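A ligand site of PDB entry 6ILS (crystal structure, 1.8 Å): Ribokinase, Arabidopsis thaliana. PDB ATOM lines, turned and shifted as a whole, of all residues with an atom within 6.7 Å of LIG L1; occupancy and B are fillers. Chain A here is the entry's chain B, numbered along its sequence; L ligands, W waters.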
ATOM      1  N   SER A  10      -1.306   7.586  14.160  1.00  0.00           N
ATOM      2  CA  SER A  10      -0.583   8.641  14.864  1.00  0.00           C
ATOM      3  C   SER A  10       0.936   8.641  14.676  1.00  0.00           C
ATOM      4  O   SER A  10       1.550   7.593  14.493  1.00  0.00           O
ATOM      5  CB  SER A  10      -0.854   8.546  16.334  1.00  0.00           C
ATOM      6  OG  SER A  10      -0.478   7.250  16.808  1.00  0.00           O
ATOM      7  N   ALA A  11       1.518   9.828  14.797  1.00  0.00           N
ATOM      8  CA  ALA A  11       2.966   9.997  14.855  1.00  0.00           C
ATOM      9  C   ALA A  11       3.257  10.961  15.994  1.00  0.00           C
ATOM     10  O   ALA A  11       2.689  12.038  16.052  1.00  0.00           O
ATOM     11  CB  ALA A  11       3.516  10.517  13.526  1.00  0.00           C
ATOM     12  N   ASN A  12       4.124  10.542  16.926  1.00  0.00           N
ATOM     13  CA  ASN A  12       4.506  11.326  18.096  1.00  0.00           C
ATOM     14  C   ASN A  12       6.007  11.482  18.205  1.00  0.00           C
ATOM     15  O   ASN A  12       6.740  10.548  17.922  1.00  0.00           O
ATOM     16  CB  ASN A  12       4.040  10.659  19.413  1.00  0.00           C
ATOM     17  CG  ASN A  12       2.551  10.659  19.587  1.00  0.00           C
ATOM     18  OD1 ASN A  12       1.853  11.569  19.135  1.00  0.00           O
ATOM     19  ND2 ASN A  12       2.044   9.641  20.288  1.00  0.00           N
ATOM     20  N   ALA A  13       6.465  12.641  18.662  1.00  0.00           N
ATOM     21  CA  ALA A  13       7.810  12.706  19.209  1.00  0.00           C
ATOM     22  C   ALA A  13       7.683  12.302  20.676  1.00  0.00           C
ATOM     23  O   ALA A  13       6.900  12.872  21.410  1.00  0.00           O
ATOM     24  CB  ALA A  13       8.409  14.110  19.064  1.00  0.00           C
ATOM     25  N   ASP A  14       8.449  11.296  21.071  1.00  0.00           N
ATOM     26  CA  ASP A  14       8.416  10.805  22.437  1.00  0.00           C
ATOM     27  C   ASP A  14       9.510  11.492  23.257  1.00  0.00           C
ATOM     28  O   ASP A  14      10.686  11.246  23.008  1.00  0.00           O
ATOM     29  CB  ASP A  14       8.579   9.291  22.452  1.00  0.00           C
ATOM     30  CG  ASP A  14       7.333   8.549  21.943  1.00  0.00           C
ATOM     31  OD1 ASP A  14       6.234   9.135  22.014  1.00  0.00           O
ATOM     32  OD2 ASP A  14       7.486   7.395  21.494  1.00  0.00           O
ATOM     33  N   TYR A  16      11.302  11.625  26.505  1.00  0.00           N
ATOM     34  CA  TYR A  16      11.620  10.887  27.720  1.00  0.00           C
ATOM     35  C   TYR A  16      12.500  11.691  28.646  1.00  0.00           C
ATOM     36  O   TYR A  16      13.556  12.145  28.242  1.00  0.00           O
ATOM     37  CB  TYR A  16      12.325   9.574  27.388  1.00  0.00           C
ATOM     38  CG  TYR A  16      11.462   8.631  26.610  1.00  0.00           C
ATOM     39  CD1 TYR A  16      10.511   7.848  27.242  1.00  0.00           C
ATOM     40  CD2 TYR A  16      11.578   8.532  25.223  1.00  0.00           C
ATOM     41  CE1 TYR A  16       9.708   6.984  26.540  1.00  0.00           C
ATOM     42  CE2 TYR A  16      10.793   7.663  24.507  1.00  0.00           C
ATOM     43  CZ  TYR A  16       9.854   6.890  25.172  1.00  0.00           C
ATOM     44  OH  TYR A  16       9.050   6.028  24.460  1.00  0.00           O
ATOM     45  N   LEU A  37      12.674  10.753  20.821  1.00  0.00           N
ATOM     46  CA  LEU A  37      12.693   9.716  19.795  1.00  0.00           C
ATOM     47  C   LEU A  37      11.411   9.720  18.954  1.00  0.00           C
ATOM     48  O   LEU A  37      10.369  10.174  19.410  1.00  0.00           O
ATOM     49  CB  LEU A  37      12.891   8.342  20.431  1.00  0.00           C
ATOM     50  CG  LEU A  37      14.223   8.043  21.140  1.00  0.00           C
ATOM     51  CD1 LEU A  37      14.129   6.737  21.910  1.00  0.00           C
ATOM     52  CD2 LEU A  37      15.363   7.976  20.128  1.00  0.00           C
ATOM     53  N   ALA A  38      11.533   9.213  17.736  1.00  0.00           N
ATOM     54  CA  ALA A  38      10.400   9.039  16.845  1.00  0.00           C
ATOM     55  C   ALA A  38       9.500   7.922  17.366  1.00  0.00           C
ATOM     56  O   ALA A  38       9.976   6.836  17.696  1.00  0.00           O
ATOM     57  CB  ALA A  38      10.864   8.730  15.455  1.00  0.00           C
ATOM     58  N   GLY A  39       8.201   8.177  17.415  1.00  0.00           N
ATOM     59  CA  GLY A  39       7.282   7.179  17.940  1.00  0.00           C
ATOM     60  C   GLY A  39       5.847   7.490  17.543  1.00  0.00           C
ATOM     61  O   GLY A  39       5.597   8.112  16.516  1.00  0.00           O
ATOM     62  N   GLY A  40       4.922   7.084  18.392  1.00  0.00           N
ATOM     63  CA  GLY A  40       3.518   7.103  18.045  1.00  0.00           C
ATOM     64  C   GLY A  40       3.112   5.723  17.571  1.00  0.00           C
ATOM     65  O   GLY A  40       3.849   5.079  16.813  1.00  0.00           O
ATOM     66  N   LYS A  41       1.918   5.269  17.953  1.00  0.00           N
ATOM     67  CA  LYS A  41       1.523   3.891  17.604  1.00  0.00           C
ATOM     68  C   LYS A  41       1.445   3.680  16.099  1.00  0.00           C
ATOM     69  O   LYS A  41       1.871   2.658  15.615  1.00  0.00           O
ATOM     70  CB  LYS A  41       0.184   3.529  18.273  1.00  0.00           C
ATOM     71  CG  LYS A  41       0.362   3.351  19.770  1.00  0.00           C
ATOM     72  CD  LYS A  41      -0.913   3.136  20.555  1.00  0.00           C
ATOM     73  CE  LYS A  41      -0.567   3.072  22.059  1.00  0.00           C
ATOM     74  NZ  LYS A  41       0.317   1.906  22.382  1.00  0.00           N
ATOM     75  N   GLY A  42       0.960   4.667  15.365  1.00  0.00           N
ATOM     76  CA  GLY A  42       0.838   4.531  13.919  1.00  0.00           C
ATOM     77  C   GLY A  42       2.202   4.502  13.252  1.00  0.00           C
ATOM     78  O   GLY A  42       2.456   3.629  12.427  1.00  0.00           O
ATOM     79  N   ASN A  44       5.036   3.785  14.613  1.00  0.00           N
ATOM     80  CA  ASN A  44       5.705   2.556  15.053  1.00  0.00           C
ATOM     81  C   ASN A  44       5.302   1.366  14.213  1.00  0.00           C
ATOM     82  O   ASN A  44       6.128   0.566  13.786  1.00  0.00           O
ATOM     83  CB  ASN A  44       5.394   2.224  16.515  1.00  0.00           C
ATOM     84  CG  ASN A  44       6.088   3.147  17.480  1.00  0.00           C
ATOM     85  OD1 ASN A  44       6.984   3.897  17.119  1.00  0.00           O
ATOM     86  ND2 ASN A  44       5.692   3.061  18.750  1.00  0.00           N
ATOM     87  N   HIS A  97       2.962  14.906  20.410  1.00  0.00           N
ATOM     88  CA  HIS A  97       4.094  14.466  21.203  1.00  0.00           C
ATOM     89  C   HIS A  97       3.623  13.961  22.556  1.00  0.00           C
ATOM     90  O   HIS A  97       2.480  14.213  22.970  1.00  0.00           O
ATOM     91  CB  HIS A  97       5.138  15.597  21.357  1.00  0.00           C
ATOM     92  CG  HIS A  97       4.569  16.935  21.708  1.00  0.00           C
ATOM     93  ND1 HIS A  97       3.870  17.707  20.809  1.00  0.00           N
ATOM     94  CD2 HIS A  97       4.645  17.659  22.853  1.00  0.00           C
ATOM     95  CE1 HIS A  97       3.501  18.838  21.398  1.00  0.00           C
ATOM     96  NE2 HIS A  97       3.971  18.843  22.632  1.00  0.00           N
ATOM     97  N   ALA A  98       4.503  13.216  23.216  1.00  0.00           N
ATOM     98  CA  ALA A  98       4.218  12.609  24.503  1.00  0.00           C
ATOM     99  C   ALA A  98       5.388  12.844  25.448  1.00  0.00           C
ATOM    100  O   ALA A  98       6.514  12.417  25.155  1.00  0.00           O
ATOM    101  CB  ALA A  98       3.950  11.122  24.346  1.00  0.00           C
ATOM    102  N   VAL A 100       7.131  11.639  28.433  1.00  0.00           N
ATOM    103  CA  VAL A 100       7.172  10.415  29.218  1.00  0.00           C
ATOM    104  C   VAL A 100       8.147  10.564  30.397  1.00  0.00           C
ATOM    105  O   VAL A 100       9.371  10.481  30.218  1.00  0.00           O
ATOM    106  CB  VAL A 100       7.581   9.203  28.348  1.00  0.00           C
ATOM    107  CG1 VAL A 100       7.493   7.922  29.146  1.00  0.00           C
ATOM    108  CG2 VAL A 100       6.701   9.135  27.115  1.00  0.00           C
ATOM    109  N   ILE A 110       2.758   9.776  31.932  1.00  0.00           N
ATOM    110  CA  ILE A 110       2.758  10.272  30.561  1.00  0.00           C
ATOM    111  C   ILE A 110       1.738  11.381  30.316  1.00  0.00           C
ATOM    112  O   ILE A 110       0.591  11.277  30.736  1.00  0.00           O
ATOM    113  CB  ILE A 110       2.519   9.118  29.571  1.00  0.00           C
ATOM    114  CG1 ILE A 110       3.668   8.111  29.647  1.00  0.00           C
ATOM    115  CG2 ILE A 110       2.369   9.639  28.134  1.00  0.00           C
ATOM    116  CD1 ILE A 110       3.682   7.063  28.577  1.00  0.00           C
ATOM    117  N   ILE A 112       0.170  13.249  26.997  1.00  0.00           N
ATOM    118  CA  ILE A 112       0.094  13.128  25.538  1.00  0.00           C
ATOM    119  C   ILE A 112      -0.556  14.354  24.916  1.00  0.00           C
ATOM    120  O   ILE A 112      -1.638  14.793  25.321  1.00  0.00           O
ATOM    121  CB  ILE A 112      -0.649  11.844  25.109  1.00  0.00           C
ATOM    122  CG1 ILE A 112       0.328  10.660  25.171  1.00  0.00           C
ATOM    123  CG2 ILE A 112      -1.219  11.978  23.698  1.00  0.00           C
ATOM    124  CD1 ILE A 112      -0.230   9.338  24.746  1.00  0.00           C
ATOM    125  N   GLU A 144      -5.331   6.744  18.418  1.00  0.00           N
ATOM    126  CA  GLU A 144      -4.572   7.977  18.684  1.00  0.00           C
ATOM    127  C   GLU A 144      -4.850   9.034  17.614  1.00  0.00           C
ATOM    128  O   GLU A 144      -4.122  10.019  17.491  1.00  0.00           O
ATOM    129  CB  GLU A 144      -3.060   7.664  18.776  1.00  0.00           C
ATOM    130  CG  GLU A 144      -2.690   6.818  19.974  1.00  0.00           C
ATOM    131  CD  GLU A 144      -1.173   6.744  20.238  1.00  0.00           C
ATOM    132  OE1 GLU A 144      -0.363   6.849  19.269  1.00  0.00           O
ATOM    133  OE2 GLU A 144      -0.796   6.601  21.422  1.00  0.00           O
ATOM    134  N   ASP A 167      -5.984  -1.728  16.575  1.00  0.00           N
ATOM    135  CA  ASP A 167      -5.244  -1.819  17.806  1.00  0.00           C
ATOM    136  C   ASP A 167      -5.963  -0.906  18.783  1.00  0.00           C
ATOM    137  O   ASP A 167      -6.325   0.215  18.415  1.00  0.00           O
ATOM    138  CB  ASP A 167      -3.779  -1.417  17.570  1.00  0.00           C
ATOM    139  CG  ASP A 167      -2.981  -1.222  18.851  1.00  0.00           C
ATOM    140  OD1 ASP A 167      -3.375  -1.731  19.908  1.00  0.00           O
ATOM    141  OD2 ASP A 167      -1.931  -0.526  18.788  1.00  0.00           O
ATOM    142  N   GLY A 170      -4.064   3.477  22.741  1.00  0.00           N
ATOM    143  CA  GLY A 170      -4.303   4.906  22.557  1.00  0.00           C
ATOM    144  C   GLY A 170      -5.281   5.414  23.616  1.00  0.00           C
ATOM    145  O   GLY A 170      -5.097   5.165  24.809  1.00  0.00           O
ATOM    146  N   THR A 255       9.032  -0.498  25.124  1.00  0.00           N
ATOM    147  CA  THR A 255       8.356   0.501  24.316  1.00  0.00           C
ATOM    148  C   THR A 255       8.308   0.072  22.830  1.00  0.00           C
ATOM    149  O   THR A 255       9.331  -0.255  22.235  1.00  0.00           O
ATOM    150  CB  THR A 255       9.033   1.882  24.426  1.00  0.00           C
ATOM    151  OG1 THR A 255       9.105   2.266  25.813  1.00  0.00           O
ATOM    152  CG2 THR A 255       8.236   2.918  23.646  1.00  0.00           C
ATOM    153  N   GLY A 256       7.099   0.084  22.264  1.00  0.00           N
ATOM    154  CA  GLY A 256       6.904  -0.243  20.870  1.00  0.00           C
ATOM    155  C   GLY A 256       6.694  -1.729  20.590  1.00  0.00           C
ATOM    156  O   GLY A 256       6.415  -2.132  19.459  1.00  0.00           O
ATOM    157  N   ALA A 257       6.817  -2.563  21.618  1.00  0.00           N
ATOM    158  CA  ALA A 257       6.725  -4.015  21.404  1.00  0.00           C
ATOM    159  C   ALA A 257       5.307  -4.479  21.050  1.00  0.00           C
ATOM    160  O   ALA A 257       5.132  -5.386  20.235  1.00  0.00           O
ATOM    161  CB  ALA A 257       7.230  -4.758  22.623  1.00  0.00           C
ATOM    162  N   GLY A 258       4.295  -3.883  21.667  1.00  0.00           N
ATOM    163  CA  GLY A 258       2.933  -4.187  21.286  1.00  0.00           C
ATOM    164  C   GLY A 258       2.668  -3.761  19.850  1.00  0.00           C
ATOM    165  O   GLY A 258       1.964  -4.438  19.113  1.00  0.00           O
ATOM    166  N   ASP A 259       3.225  -2.619  19.460  1.00  0.00           N
ATOM    167  CA  ASP A 259       3.085  -2.139  18.083  1.00  0.00           C
ATOM    168  C   ASP A 259       3.759  -3.089  17.113  1.00  0.00           C
ATOM    169  O   ASP A 259       3.226  -3.392  16.046  1.00  0.00           O
ATOM    170  CB  ASP A 259       3.686  -0.737  17.948  1.00  0.00           C
ATOM    171  CG  ASP A 259       2.918   0.301  18.758  1.00  0.00           C
ATOM    172  OD1 ASP A 259       1.680   0.218  18.746  1.00  0.00           O
ATOM    173  OD2 ASP A 259       3.559   1.160  19.398  1.00  0.00           O
ATOM    174  N   ALA A 295      11.536   2.900  20.375  1.00  0.00           N
ATOM    175  CA  ALA A 295      10.503   2.198  19.605  1.00  0.00           C
ATOM    176  C   ALA A 295      11.005   1.853  18.199  1.00  0.00           C
ATOM    177  O   ALA A 295      11.397   0.723  17.921  1.00  0.00           O
ATOM    178  CB  ALA A 295       9.217   3.021  19.528  1.00  0.00           C
HETATM  179  O1  LIG L   1       3.104   2.172  21.654  1.00  0.00           O
HETATM  180  C1  LIG L   1       4.120   3.145  21.769  1.00  0.00           C
HETATM  181  C2  LIG L   1       3.603   4.409  21.525  1.00  0.00           C
HETATM  182  O2  LIG L   1       2.414   4.731  22.385  1.00  0.00           O
HETATM  183  C3  LIG L   1       4.717   5.432  22.038  1.00  0.00           C
HETATM  184  O3  LIG L   1       5.687   5.655  20.911  1.00  0.00           O
HETATM  185  C4  LIG L   1       4.106   6.434  22.480  1.00  0.00           C
HETATM  186  O4  LIG L   1       4.278   7.640  21.649  1.00  0.00           O
HETATM  187  C5  LIG L   1       2.487   6.024  22.599  1.00  0.00           C
HETATM  188  O5  LIG L   1       1.754   6.711  21.650  1.00  0.00           O
HETATM  189  P1  LG2 L   2       0.636  -3.612  24.610  1.00  0.00           P
HETATM  190  O1  LG2 L   2      -0.415  -3.422  23.567  1.00  0.00           O
HETATM  191  O2  LG2 L   2       1.868  -2.783  24.275  1.00  0.00           O
HETATM  192  O3  LG2 L   2       0.153  -3.150  25.951  1.00  0.00           O
HETATM  193  P2  LG2 L   2       1.263  -5.986  25.952  1.00  0.00           P
HETATM  194  O4  LG2 L   2       1.530  -7.389  25.595  1.00  0.00           O
HETATM  195  O5  LG2 L   2       0.125  -5.988  26.861  1.00  0.00           O
HETATM  196  O6  LG2 L   2       0.959  -5.178  24.639  1.00  0.00           O
HETATM  197  P3  LG2 L   2       3.967  -5.622  26.963  1.00  0.00           P
HETATM  198  O7  LG2 L   2       4.066  -6.434  28.252  1.00  0.00           O
HETATM  199  O8  LG2 L   2       4.820  -4.385  27.070  1.00  0.00           O
HETATM  200  O9  LG2 L   2       2.464  -5.211  26.708  1.00  0.00           O
HETATM  201  O10 LG2 L   2       4.509  -6.491  25.782  1.00  0.00           O
HETATM  202  C1  LG2 L   2       4.425  -6.011  24.450  1.00  0.00           C
HETATM  203  C2  LG2 L   2       4.836  -7.214  23.489  1.00  0.00           C
HETATM  204  O11 LG2 L   2       6.237  -7.720  23.878  1.00  0.00           O
HETATM  205  C3  LG2 L   2       4.041  -8.182  23.669  1.00  0.00           C
HETATM  206  O12 LG2 L   2       3.774  -8.844  22.422  1.00  0.00           O
HETATM  207  C4  LG2 L   2       4.797  -9.250  24.686  1.00  0.00           C
HETATM  208  O13 LG2 L   2       4.198 -10.553  24.462  1.00  0.00           O
HETATM  209  C5  LG2 L   2       6.027  -9.168  24.406  1.00  0.00           C
HETATM  210  N1  LG2 L   2       6.842  -9.239  25.641  1.00  0.00           N
HETATM  211  C6  LG2 L   2       6.861  -8.701  26.889  1.00  0.00           C
HETATM  212  N2  LG2 L   2       7.927  -9.229  27.552  1.00  0.00           N
HETATM  213  C7  LG2 L   2       8.569 -10.078  26.698  1.00  0.00           C
HETATM  214  C8  LG2 L   2       9.715 -10.870  26.866  1.00  0.00           C
HETATM  215  N3  LG2 L   2      10.536 -10.995  28.034  1.00  0.00           N
HETATM  216  N4  LG2 L   2      10.133 -11.631  25.859  1.00  0.00           N
HETATM  217  C9  LG2 L   2       9.462 -11.630  24.647  1.00  0.00           C
HETATM  218  N5  LG2 L   2       8.359 -10.867  24.474  1.00  0.00           N
HETATM  219  C10 LG2 L   2       7.911 -10.088  25.511  1.00  0.00           C
HETATM  220  O   HOH W   1       3.872  -0.809  21.790  1.00  0.00           O
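OD1 of Asp 14 lies within hydrogen-bond range of O4 of LIG L1 (2.5 Å).
OD2 of Asp 259 lies within hydrogen-bond range of O1 of LIG L1 (2.5 Å).
OE2 of Glu 144 is in hydrogen-bond range of O5 of LIG L1 (2.6 Å).
O1 of LIG L1 is in hydrogen-bond range of NZ of Lys 41, 2.9 Å away.
O3 of LIG L1 lies within hydrogen-bond range of N of Gly 40.
ND2 of Asn 12 lies within hydrogen-bond range of O5 of LIG L1 (3.2 Å).
The side-chain amide nitrogen (ND2) of Asn 44 lies within hydrogen-bond range of an oxygen (O3) of LIG L1, at 3.4 Å.
The backbone NH of Asp 14 lies within hydrogen-bond range of the backbone carbonyl oxygen of Leu 37, at 2.8 Å.
OD2 of Asp 259 lies within hydrogen-bond range of ND2 of Asn 44 (2.9 Å).
OE1 of Glu 144 lies within hydrogen-bond range of N of Lys 41 (3.1 Å).
The side-chain carboxylate (OE1) of Glu 144 lies within hydrogen-bond range of the side-chain hydroxyl (OG) of Ser 10 (2.5 Å).
The backbone NH of Lys 41 lies within hydrogen-bond range of the side-chain hydroxyl of Ser 10, at 3.3 Å.
The backbone carbonyl oxygen (O) of Gly 40 sits close to the side-chain amide nitrogen (ND2) of Asn 44, at 3.3 Å.
The backbone NH of Gly 39 sits at hydrogen-bond distance from the backbone carbonyl oxygen of Asn 12, 2.8 Å away.
CA of Gly 39 touches O3 of LIG L1, 3.7 Å away.
The nearest printed residue that does not touch LIG L1 is Gly 256 (4.3 Å).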
